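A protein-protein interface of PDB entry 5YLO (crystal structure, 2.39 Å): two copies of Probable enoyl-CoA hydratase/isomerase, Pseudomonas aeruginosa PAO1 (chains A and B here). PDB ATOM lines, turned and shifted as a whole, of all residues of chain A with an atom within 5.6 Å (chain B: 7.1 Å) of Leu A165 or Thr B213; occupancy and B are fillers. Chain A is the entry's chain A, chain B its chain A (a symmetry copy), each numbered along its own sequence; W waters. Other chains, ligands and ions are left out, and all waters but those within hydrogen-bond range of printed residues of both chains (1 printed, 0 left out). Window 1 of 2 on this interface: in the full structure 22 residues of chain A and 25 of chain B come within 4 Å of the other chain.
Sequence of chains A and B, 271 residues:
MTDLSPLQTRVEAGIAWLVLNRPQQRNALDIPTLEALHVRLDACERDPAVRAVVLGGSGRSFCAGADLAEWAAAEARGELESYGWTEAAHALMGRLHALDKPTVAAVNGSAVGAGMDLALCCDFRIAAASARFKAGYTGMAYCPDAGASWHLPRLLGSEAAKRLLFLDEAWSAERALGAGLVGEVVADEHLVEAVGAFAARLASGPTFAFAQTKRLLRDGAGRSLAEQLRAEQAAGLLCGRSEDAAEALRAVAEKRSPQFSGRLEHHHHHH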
ATOM      1  N   ALA A 135      18.998  11.876 -15.434  1.00  0.00           N
ATOM      2  CA  ALA A 135      18.256  10.645 -15.202  1.00  0.00           C
ATOM      3  C   ALA A 135      19.182   9.600 -14.601  1.00  0.00           C
ATOM      4  O   ALA A 135      20.380   9.571 -14.891  1.00  0.00           O
ATOM      5  CB  ALA A 135      17.641  10.098 -16.491  1.00  0.00           C
ATOM      6  N   GLY A 136      18.610   8.735 -13.778  1.00  0.00           N
ATOM      7  CA  GLY A 136      19.370   7.619 -13.245  1.00  0.00           C
ATOM      8  C   GLY A 136      20.456   8.101 -12.313  1.00  0.00           C
ATOM      9  O   GLY A 136      20.191   8.777 -11.314  1.00  0.00           O
ATOM     10  N   TYR A 137      21.702   7.768 -12.642  1.00  0.00           N
ATOM     11  CA  TYR A 137      22.840   8.168 -11.821  1.00  0.00           C
ATOM     12  C   TYR A 137      23.085   9.667 -11.961  1.00  0.00           C
ATOM     13  O   TYR A 137      23.284  10.169 -13.071  1.00  0.00           O
ATOM     14  CB  TYR A 137      24.072   7.370 -12.238  1.00  0.00           C
ATOM     15  CG  TYR A 137      25.322   7.631 -11.419  1.00  0.00           C
ATOM     16  CD1 TYR A 137      25.268   7.728 -10.035  1.00  0.00           C
ATOM     17  CD2 TYR A 137      26.564   7.748 -12.035  1.00  0.00           C
ATOM     18  CE1 TYR A 137      26.412   7.955  -9.290  1.00  0.00           C
ATOM     19  CE2 TYR A 137      27.710   7.974 -11.298  1.00  0.00           C
ATOM     20  CZ  TYR A 137      27.630   8.075  -9.926  1.00  0.00           C
ATOM     21  OH  TYR A 137      28.770   8.300  -9.188  1.00  0.00           O
ATOM     22  N   TYR A 142      20.588   8.465  -7.111  1.00  0.00           N
ATOM     23  CA  TYR A 142      20.050   7.673  -8.213  1.00  0.00           C
ATOM     24  C   TYR A 142      18.536   7.826  -8.227  1.00  0.00           C
ATOM     25  O   TYR A 142      17.863   7.445  -7.264  1.00  0.00           O
ATOM     26  CB  TYR A 142      20.446   6.199  -8.079  1.00  0.00           C
ATOM     27  CG  TYR A 142      20.391   5.434  -9.379  1.00  0.00           C
ATOM     28  CD1 TYR A 142      19.192   4.916  -9.854  1.00  0.00           C
ATOM     29  CD2 TYR A 142      21.538   5.229 -10.133  1.00  0.00           C
ATOM     30  CE1 TYR A 142      19.138   4.218 -11.042  1.00  0.00           C
ATOM     31  CE2 TYR A 142      21.495   4.530 -11.323  1.00  0.00           C
ATOM     32  CZ  TYR A 142      20.292   4.027 -11.772  1.00  0.00           C
ATOM     33  OH  TYR A 142      20.242   3.331 -12.957  1.00  0.00           O
ATOM     34  N   ASP A 145      13.850   4.875 -11.666  1.00  0.00           N
ATOM     35  CA  ASP A 145      14.106   4.531 -13.058  1.00  0.00           C
ATOM     36  C   ASP A 145      12.978   3.724 -13.690  1.00  0.00           C
ATOM     37  O   ASP A 145      13.165   3.169 -14.776  1.00  0.00           O
ATOM     38  CB  ASP A 145      15.428   3.765 -13.173  1.00  0.00           C
ATOM     39  CG  ASP A 145      15.456   2.512 -12.310  1.00  0.00           C
ATOM     40  OD1 ASP A 145      14.784   2.496 -11.258  1.00  0.00           O
ATOM     41  OD2 ASP A 145      16.152   1.544 -12.681  1.00  0.00           O
ATOM     42  N   ALA A 148      11.591   5.997 -16.551  1.00  0.00           N
ATOM     43  CA  ALA A 148      12.730   6.290 -17.414  1.00  0.00           C
ATOM     44  C   ALA A 148      13.122   5.067 -18.236  1.00  0.00           C
ATOM     45  O   ALA A 148      13.326   5.159 -19.453  1.00  0.00           O
ATOM     46  CB  ALA A 148      13.911   6.783 -16.578  1.00  0.00           C
ATOM     47  N   SER A 149      13.212   3.901 -17.588  1.00  0.00           N
ATOM     48  CA  SER A 149      13.574   2.675 -18.292  1.00  0.00           C
ATOM     49  C   SER A 149      12.510   2.244 -19.290  1.00  0.00           C
ATOM     50  O   SER A 149      12.782   1.393 -20.143  1.00  0.00           O
ATOM     51  CB  SER A 149      13.828   1.547 -17.291  1.00  0.00           C
ATOM     52  OG  SER A 149      12.624   1.173 -16.646  1.00  0.00           O
ATOM     53  N   LEU A 152      12.722   6.122 -22.021  1.00  0.00           N
ATOM     54  CA  LEU A 152      13.980   6.498 -22.665  1.00  0.00           C
ATOM     55  C   LEU A 152      14.392   5.568 -23.800  1.00  0.00           C
ATOM     56  O   LEU A 152      14.780   6.076 -24.866  1.00  0.00           O
ATOM     57  CB  LEU A 152      15.084   6.612 -21.609  1.00  0.00           C
ATOM     58  CG  LEU A 152      14.951   7.773 -20.625  1.00  0.00           C
ATOM     59  CD1 LEU A 152      16.136   7.802 -19.672  1.00  0.00           C
ATOM     60  CD2 LEU A 152      14.824   9.088 -21.378  1.00  0.00           C
ATOM     61  N   ALA A 160      21.625   4.956 -26.264  1.00  0.00           N
ATOM     62  CA  ALA A 160      21.532   6.355 -25.858  1.00  0.00           C
ATOM     63  C   ALA A 160      20.818   6.492 -24.521  1.00  0.00           C
ATOM     64  O   ALA A 160      21.201   7.320 -23.686  1.00  0.00           O
ATOM     65  CB  ALA A 160      20.819   7.169 -26.937  1.00  0.00           C
ATOM     66  N   ALA A 161      19.782   5.681 -24.297  1.00  0.00           N
ATOM     67  CA  ALA A 161      19.096   5.688 -23.011  1.00  0.00           C
ATOM     68  C   ALA A 161      20.005   5.215 -21.886  1.00  0.00           C
ATOM     69  O   ALA A 161      19.880   5.689 -20.751  1.00  0.00           O
ATOM     70  CB  ALA A 161      17.841   4.818 -23.080  1.00  0.00           C
ATOM     71  N   LYS A 162      20.924   4.292 -22.176  1.00  0.00           N
ATOM     72  CA  LYS A 162      21.828   3.805 -21.141  1.00  0.00           C
ATOM     73  C   LYS A 162      22.955   4.790 -20.859  1.00  0.00           C
ATOM     74  O   LYS A 162      23.478   4.818 -19.741  1.00  0.00           O
ATOM     75  CB  LYS A 162      22.394   2.440 -21.534  1.00  0.00           C
ATOM     76  CG  LYS A 162      21.342   1.344 -21.616  1.00  0.00           C
ATOM     77  CD  LYS A 162      21.931   0.042 -22.125  1.00  0.00           C
ATOM     78  CE  LYS A 162      20.854  -1.011 -22.302  1.00  0.00           C
ATOM     79  NZ  LYS A 162      21.404  -2.245 -22.922  1.00  0.00           N
ATOM     80  N   ARG A 163      23.342   5.601 -21.848  1.00  0.00           N
ATOM     81  CA  ARG A 163      24.303   6.667 -21.581  1.00  0.00           C
ATOM     82  C   ARG A 163      23.727   7.684 -20.607  1.00  0.00           C
ATOM     83  O   ARG A 163      24.410   8.119 -19.673  1.00  0.00           O
ATOM     84  CB  ARG A 163      24.717   7.354 -22.884  1.00  0.00           C
ATOM     85  CG  ARG A 163      25.674   6.550 -23.746  1.00  0.00           C
ATOM     86  CD  ARG A 163      26.195   7.362 -24.923  1.00  0.00           C
ATOM     87  NE  ARG A 163      27.024   6.546 -25.806  1.00  0.00           N
ATOM     88  CZ  ARG A 163      28.339   6.399 -25.673  1.00  0.00           C
ATOM     89  NH1 ARG A 163      28.983   7.017 -24.693  1.00  0.00           N
ATOM     90  NH2 ARG A 163      29.011   5.633 -26.522  1.00  0.00           N
ATOM     91  N   LEU A 164      22.463   8.064 -20.803  1.00  0.00           N
ATOM     92  CA  LEU A 164      21.841   9.060 -19.939  1.00  0.00           C
ATOM     93  C   LEU A 164      21.605   8.513 -18.536  1.00  0.00           C
ATOM     94  O   LEU A 164      21.748   9.241 -17.547  1.00  0.00           O
ATOM     95  CB  LEU A 164      20.528   9.535 -20.559  1.00  0.00           C
ATOM     96  CG  LEU A 164      19.751  10.588 -19.770  1.00  0.00           C
ATOM     97  CD1 LEU A 164      20.633  11.797 -19.505  1.00  0.00           C
ATOM     98  CD2 LEU A 164      18.488  10.989 -20.516  1.00  0.00           C
ATOM     99  N   LEU A 165      21.245   7.234 -18.428  1.00  0.00           N
ATOM    100  CA  LEU A 165      20.947   6.660 -17.120  1.00  0.00           C
ATOM    101  C   LEU A 165      22.214   6.298 -16.352  1.00  0.00           C
ATOM    102  O   LEU A 165      22.296   6.545 -15.143  1.00  0.00           O
ATOM    103  CB  LEU A 165      20.051   5.432 -17.279  1.00  0.00           C
ATOM    104  CG  LEU A 165      18.576   5.704 -17.579  1.00  0.00           C
ATOM    105  CD1 LEU A 165      17.896   4.458 -18.131  1.00  0.00           C
ATOM    106  CD2 LEU A 165      17.859   6.195 -16.329  1.00  0.00           C
ATOM    107  N   PHE A 166      23.209   5.716 -17.021  1.00  0.00           N
ATOM    108  CA  PHE A 166      24.378   5.209 -16.312  1.00  0.00           C
ATOM    109  C   PHE A 166      25.443   6.271 -16.078  1.00  0.00           C
ATOM    110  O   PHE A 166      26.149   6.211 -15.066  1.00  0.00           O
ATOM    111  CB  PHE A 166      24.992   4.027 -17.070  1.00  0.00           C
ATOM    112  CG  PHE A 166      24.092   2.823 -17.155  1.00  0.00           C
ATOM    113  CD1 PHE A 166      22.957   2.726 -16.364  1.00  0.00           C
ATOM    114  CD2 PHE A 166      24.386   1.782 -18.021  1.00  0.00           C
ATOM    115  CE1 PHE A 166      22.131   1.620 -16.442  1.00  0.00           C
ATOM    116  CE2 PHE A 166      23.564   0.672 -18.102  1.00  0.00           C
ATOM    117  CZ  PHE A 166      22.435   0.592 -17.312  1.00  0.00           C
ATOM    118  N   LEU A 167      25.580   7.239 -16.978  1.00  0.00           N
ATOM    119  CA  LEU A 167      26.500   8.341 -16.754  1.00  0.00           C
ATOM    120  C   LEU A 167      25.821   9.436 -15.943  1.00  0.00           C
ATOM    121  O   LEU A 167      24.609   9.645 -16.032  1.00  0.00           O
ATOM    122  CB  LEU A 167      26.998   8.913 -18.080  1.00  0.00           C
ATOM    123  CG  LEU A 167      27.650   7.912 -19.031  1.00  0.00           C
ATOM    124  CD1 LEU A 167      28.192   8.630 -20.252  1.00  0.00           C
ATOM    125  CD2 LEU A 167      28.748   7.145 -18.315  1.00  0.00           C
ATOM    126  N   THR B 207      26.948  -0.075  -9.319  1.00  0.00           N
ATOM    127  CA  THR B 207      26.740  -1.241 -10.172  1.00  0.00           C
ATOM    128  C   THR B 207      25.408  -1.920  -9.869  1.00  0.00           C
ATOM    129  O   THR B 207      24.744  -2.434 -10.779  1.00  0.00           O
ATOM    130  CB  THR B 207      27.898  -2.226 -10.005  1.00  0.00           C
ATOM    131  OG1 THR B 207      29.140  -1.540 -10.197  1.00  0.00           O
ATOM    132  CG2 THR B 207      27.792  -3.355 -11.020  1.00  0.00           C
ATOM    133  N   PHE B 208      25.000  -1.926  -8.599  1.00  0.00           N
ATOM    134  CA  PHE B 208      23.746  -2.571  -8.219  1.00  0.00           C
ATOM    135  C   PHE B 208      22.552  -1.893  -8.879  1.00  0.00           C
ATOM    136  O   PHE B 208      21.624  -2.566  -9.345  1.00  0.00           O
ATOM    137  CB  PHE B 208      23.597  -2.564  -6.695  1.00  0.00           C
ATOM    138  CG  PHE B 208      23.638  -1.182  -6.079  1.00  0.00           C
ATOM    139  CD1 PHE B 208      24.848  -0.558  -5.809  1.00  0.00           C
ATOM    140  CD2 PHE B 208      22.463  -0.513  -5.760  1.00  0.00           C
ATOM    141  CE1 PHE B 208      24.888   0.709  -5.242  1.00  0.00           C
ATOM    142  CE2 PHE B 208      22.498   0.756  -5.193  1.00  0.00           C
ATOM    143  CZ  PHE B 208      23.712   1.365  -4.934  1.00  0.00           C
ATOM    144  N   ALA B 209      22.554  -0.560  -8.922  1.00  0.00           N
ATOM    145  CA  ALA B 209      21.444   0.159  -9.534  1.00  0.00           C
ATOM    146  C   ALA B 209      21.416  -0.058 -11.040  1.00  0.00           C
ATOM    147  O   ALA B 209      20.339  -0.162 -11.638  1.00  0.00           O
ATOM    148  CB  ALA B 209      21.537   1.647  -9.202  1.00  0.00           C
ATOM    149  N   PHE B 210      22.592  -0.136 -11.668  1.00  0.00           N
ATOM    150  CA  PHE B 210      22.643  -0.404 -13.102  1.00  0.00           C
ATOM    151  C   PHE B 210      22.043  -1.766 -13.422  1.00  0.00           C
ATOM    152  O   PHE B 210      21.350  -1.926 -14.435  1.00  0.00           O
ATOM    153  CB  PHE B 210      24.086  -0.327 -13.609  1.00  0.00           C
ATOM    154  CG  PHE B 210      24.755   1.005 -13.378  1.00  0.00           C
ATOM    155  CD1 PHE B 210      24.014   2.150 -13.127  1.00  0.00           C
ATOM    156  CD2 PHE B 210      26.138   1.110 -13.426  1.00  0.00           C
ATOM    157  CE1 PHE B 210      24.641   3.368 -12.919  1.00  0.00           C
ATOM    158  CE2 PHE B 210      26.768   2.323 -13.219  1.00  0.00           C
ATOM    159  CZ  PHE B 210      26.018   3.454 -12.967  1.00  0.00           C
ATOM    160  N   ALA B 211      22.290  -2.760 -12.564  1.00  0.00           N
ATOM    161  CA  ALA B 211      21.763  -4.099 -12.799  1.00  0.00           C
ATOM    162  C   ALA B 211      20.240  -4.097 -12.785  1.00  0.00           C
ATOM    163  O   ALA B 211      19.599  -4.664 -13.678  1.00  0.00           O
ATOM    164  CB  ALA B 211      22.312  -5.070 -11.753  1.00  0.00           C
ATOM    165  N   GLN B 212      19.643  -3.461 -11.776  1.00  0.00           N
ATOM    166  CA  GLN B 212      18.188  -3.357 -11.732  1.00  0.00           C
ATOM    167  C   GLN B 212      17.662  -2.536 -12.902  1.00  0.00           C
ATOM    168  O   GLN B 212      16.645  -2.890 -13.509  1.00  0.00           O
ATOM    169  CB  GLN B 212      17.742  -2.743 -10.407  1.00  0.00           C
ATOM    170  CG  GLN B 212      18.017  -3.611  -9.196  1.00  0.00           C
ATOM    171  CD  GLN B 212      17.549  -2.968  -7.906  1.00  0.00           C
ATOM    172  OE1 GLN B 212      17.925  -1.839  -7.588  1.00  0.00           O
ATOM    173  NE2 GLN B 212      16.717  -3.682  -7.156  1.00  0.00           N
ATOM    174  N   THR B 213      18.343  -1.437 -13.231  1.00  0.00           N
ATOM    175  CA  THR B 213      17.922  -0.611 -14.361  1.00  0.00           C
ATOM    176  C   THR B 213      18.022  -1.376 -15.673  1.00  0.00           C
ATOM    177  O   THR B 213      17.131  -1.280 -16.526  1.00  0.00           O
ATOM    178  CB  THR B 213      18.761   0.666 -14.418  1.00  0.00           C
ATOM    179  OG1 THR B 213      18.384   1.537 -13.343  1.00  0.00           O
ATOM    180  CG2 THR B 213      18.565   1.390 -15.746  1.00  0.00           C
ATOM    181  N   LYS B 214      19.096  -2.149 -15.853  1.00  0.00           N
ATOM    182  CA  LYS B 214      19.257  -2.903 -17.092  1.00  0.00           C
ATOM    183  C   LYS B 214      18.173  -3.964 -17.235  1.00  0.00           C
ATOM    184  O   LYS B 214      17.705  -4.239 -18.347  1.00  0.00           O
ATOM    185  CB  LYS B 214      20.650  -3.530 -17.150  1.00  0.00           C
ATOM    186  CG  LYS B 214      20.955  -4.237 -18.459  1.00  0.00           C
ATOM    187  CD  LYS B 214      22.422  -4.621 -18.564  1.00  0.00           C
ATOM    188  CE  LYS B 214      22.683  -5.441 -19.817  1.00  0.00           C
ATOM    189  NZ  LYS B 214      24.138  -5.700 -20.018  1.00  0.00           N
ATOM    190  N   ARG B 215      17.752  -4.566 -16.119  1.00  0.00           N
ATOM    191  CA  ARG B 215      16.644  -5.516 -16.168  1.00  0.00           C
ATOM    192  C   ARG B 215      15.322  -4.826 -16.477  1.00  0.00           C
ATOM    193  O   ARG B 215      14.468  -5.402 -17.160  1.00  0.00           O
ATOM    194  CB  ARG B 215      16.543  -6.280 -14.848  1.00  0.00           C
ATOM    195  CG  ARG B 215      17.429  -7.514 -14.759  1.00  0.00           C
ATOM    196  CD  ARG B 215      17.156  -8.287 -13.477  1.00  0.00           C
ATOM    197  NE  ARG B 215      17.790  -7.674 -12.313  1.00  0.00           N
ATOM    198  CZ  ARG B 215      18.748  -8.253 -11.597  1.00  0.00           C
ATOM    199  NH1 ARG B 215      19.173  -9.469 -11.914  1.00  0.00           N
ATOM    200  NH2 ARG B 215      19.272  -7.623 -10.555  1.00  0.00           N
ATOM    201  N   LEU B 216      15.133  -3.599 -15.987  1.00  0.00           N
ATOM    202  CA  LEU B 216      13.890  -2.882 -16.251  1.00  0.00           C
ATOM    203  C   LEU B 216      13.807  -2.437 -17.704  1.00  0.00           C
ATOM    204  O   LEU B 216      12.735  -2.509 -18.319  1.00  0.00           O
ATOM    205  CB  LEU B 216      13.770  -1.684 -15.312  1.00  0.00           C
ATOM    206  CG  LEU B 216      13.438  -2.009 -13.855  1.00  0.00           C
ATOM    207  CD1 LEU B 216      13.650  -0.788 -12.979  1.00  0.00           C
ATOM    208  CD2 LEU B 216      12.007  -2.514 -13.731  1.00  0.00           C
ATOM    209  N   LEU B 217      14.924  -1.961 -18.265  1.00  0.00           N
ATOM    210  CA  LEU B 217      14.953  -1.605 -19.681  1.00  0.00           C
ATOM    211  C   LEU B 217      14.533  -2.786 -20.543  1.00  0.00           C
ATOM    212  O   LEU B 217      13.701  -2.651 -21.447  1.00  0.00           O
ATOM    213  CB  LEU B 217      16.354  -1.135 -20.078  1.00  0.00           C
ATOM    214  CG  LEU B 217      16.879   0.195 -19.538  1.00  0.00           C
ATOM    215  CD1 LEU B 217      18.391   0.231 -19.651  1.00  0.00           C
ATOM    216  CD2 LEU B 217      16.265   1.353 -20.303  1.00  0.00           C
ATOM    217  N   ARG B 218      15.099  -3.961 -20.265  1.00  0.00           N
ATOM    218  CA  ARG B 218      14.820  -5.141 -21.073  1.00  0.00           C
ATOM    219  C   ARG B 218      13.386  -5.618 -20.874  1.00  0.00           C
ATOM    220  O   ARG B 218      12.667  -5.872 -21.848  1.00  0.00           O
ATOM    221  CB  ARG B 218      15.821  -6.245 -20.727  1.00  0.00           C
ATOM    222  CG  ARG B 218      15.733  -7.493 -21.585  1.00  0.00           C
ATOM    223  CD  ARG B 218      16.917  -8.419 -21.325  1.00  0.00           C
ATOM    224  NE  ARG B 218      17.044  -8.780 -19.913  1.00  0.00           N
ATOM    225  CZ  ARG B 218      17.954  -8.271 -19.087  1.00  0.00           C
ATOM    226  NH1 ARG B 218      18.830  -7.377 -19.527  1.00  0.00           N
ATOM    227  NH2 ARG B 218      17.991  -8.660 -17.820  1.00  0.00           N
ATOM    228  N   ASP B 219      12.946  -5.735 -19.618  1.00  0.00           N
ATOM    229  CA  ASP B 219      11.580  -6.177 -19.360  1.00  0.00           C
ATOM    230  C   ASP B 219      10.555  -5.167 -19.864  1.00  0.00           C
ATOM    231  O   ASP B 219       9.466  -5.557 -20.299  1.00  0.00           O
ATOM    232  CB  ASP B 219      11.374  -6.430 -17.865  1.00  0.00           C
ATOM    233  CG  ASP B 219      12.119  -7.655 -17.363  1.00  0.00           C
ATOM    234  OD1 ASP B 219      12.612  -8.441 -18.199  1.00  0.00           O
ATOM    235  OD2 ASP B 219      12.203  -7.833 -16.128  1.00  0.00           O
ATOM    236  N   GLN B 228       4.789  -1.647 -16.427  1.00  0.00           N
ATOM    237  CA  GLN B 228       6.152  -1.362 -15.992  1.00  0.00           C
ATOM    238  C   GLN B 228       6.163  -0.699 -14.621  1.00  0.00           C
ATOM    239  O   GLN B 228       6.990  -1.035 -13.765  1.00  0.00           O
ATOM    240  CB  GLN B 228       6.853  -0.480 -17.028  1.00  0.00           C
ATOM    241  CG  GLN B 228       8.260  -0.031 -16.647  1.00  0.00           C
ATOM    242  CD  GLN B 228       9.337  -1.006 -17.093  1.00  0.00           C
ATOM    243  OE1 GLN B 228       9.115  -2.214 -17.144  1.00  0.00           O
ATOM    244  NE2 GLN B 228      10.510  -0.478 -17.425  1.00  0.00           N
HETATM  245  O   HOH W   1      11.589  -0.419 -21.721  1.00  0.00           O
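Leu A165 touches just one residue of chain B: Thr B213 (3.9 Å). Thr B213 touches four residues of chain A. Of the printed residues of chain A, Gln B228 touches Ser A149. Printed residues of chain B within 4 Å of Asp A145: Thr B213 (2.3 Å) and Leu B216 (3.4 Å). Printed residues of chain B within 4 Å of Tyr A142: Ala B209 (3.6 Å), Phe B210 (3.7 Å) and Thr B213 (2.6 Å). Of the printed residues of chain A, Leu B216 touches Asp A145 and Ser A149. Printed residues of chain B within 4 Å of Phe A166: Phe B210 (3.5 Å) and Thr B213 (3.6 Å). Leu A167 touches none of the printed residues of chain B. Ala B211 touches none of the printed residues of chain A.
O of Ala B209 lies within hydrogen-bond range of OG1 of Thr B213, 3.1 Å away. The side-chain hydroxyl of Ser A149 sits at hydrogen-bond distance from the backbone carbonyl oxygen of Asp A145 (2.8 Å). NE2 of Gln B228 is in hydrogen-bond range of O of Leu B216 (3.1 Å). N of Tyr A137 lies within hydrogen-bond range of O of Leu A165.
The side-chain hydroxyl (OH) of Tyr A142 lies within hydrogen-bond range of the side-chain hydroxyl (OG1) of Thr B213, 2.6 Å away. OD2 of Asp A145 lies close to OG1 of Thr B213. NE2 of Gln B228 sits at hydrogen-bond distance from OG of Ser A149.
No position is printed for both chains.
Hydrophobic or aromatic side chains of chain A that line the printed part of chain B: Tyr A142, Leu A165 and Phe A166. Of the 14 printed residues of chain B, 6 touch a printed residue of chain A. Hydrophobic or aromatic side chains of chain B that line the printed part of chain A: Ala B209, Phe B210, Leu B216 and Leu B217. Among the printed residues, no Asp or Glu carboxylate lies within 4 Å of a Lys or Arg side-chain nitrogen of the other chain.
Water W1 lies within hydrogen-bond range of the backbone carbonyl oxygen (O) of Ser A149 (2.7 Å) and the backbone carbonyl oxygen (O) of Leu B217 (3.1 Å).
Tyr A142 touches Ala B209. CE2 of Tyr A142 touches CE1 of Phe B210 (3.7 Å). Leu B216 touches Asp A145 (CD1 to OD2, 3.4 Å). CB of Leu B216 touches OG of Ser A149, 3.4 Å away. Leu B217 touches Ser A149 (CD2 to O, 3.5 Å). CG of Lys A162 touches CD1 of Leu B217 (3.7 Å). CD1 of Leu A165 touches CG2 of Thr B213, at 3.9 Å. Phe B210 touches Phe A166 (CD1 to CD1, 3.5 Å). CG2 of Thr B213 touches CE1 of Phe A166, 3.6 Å away.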
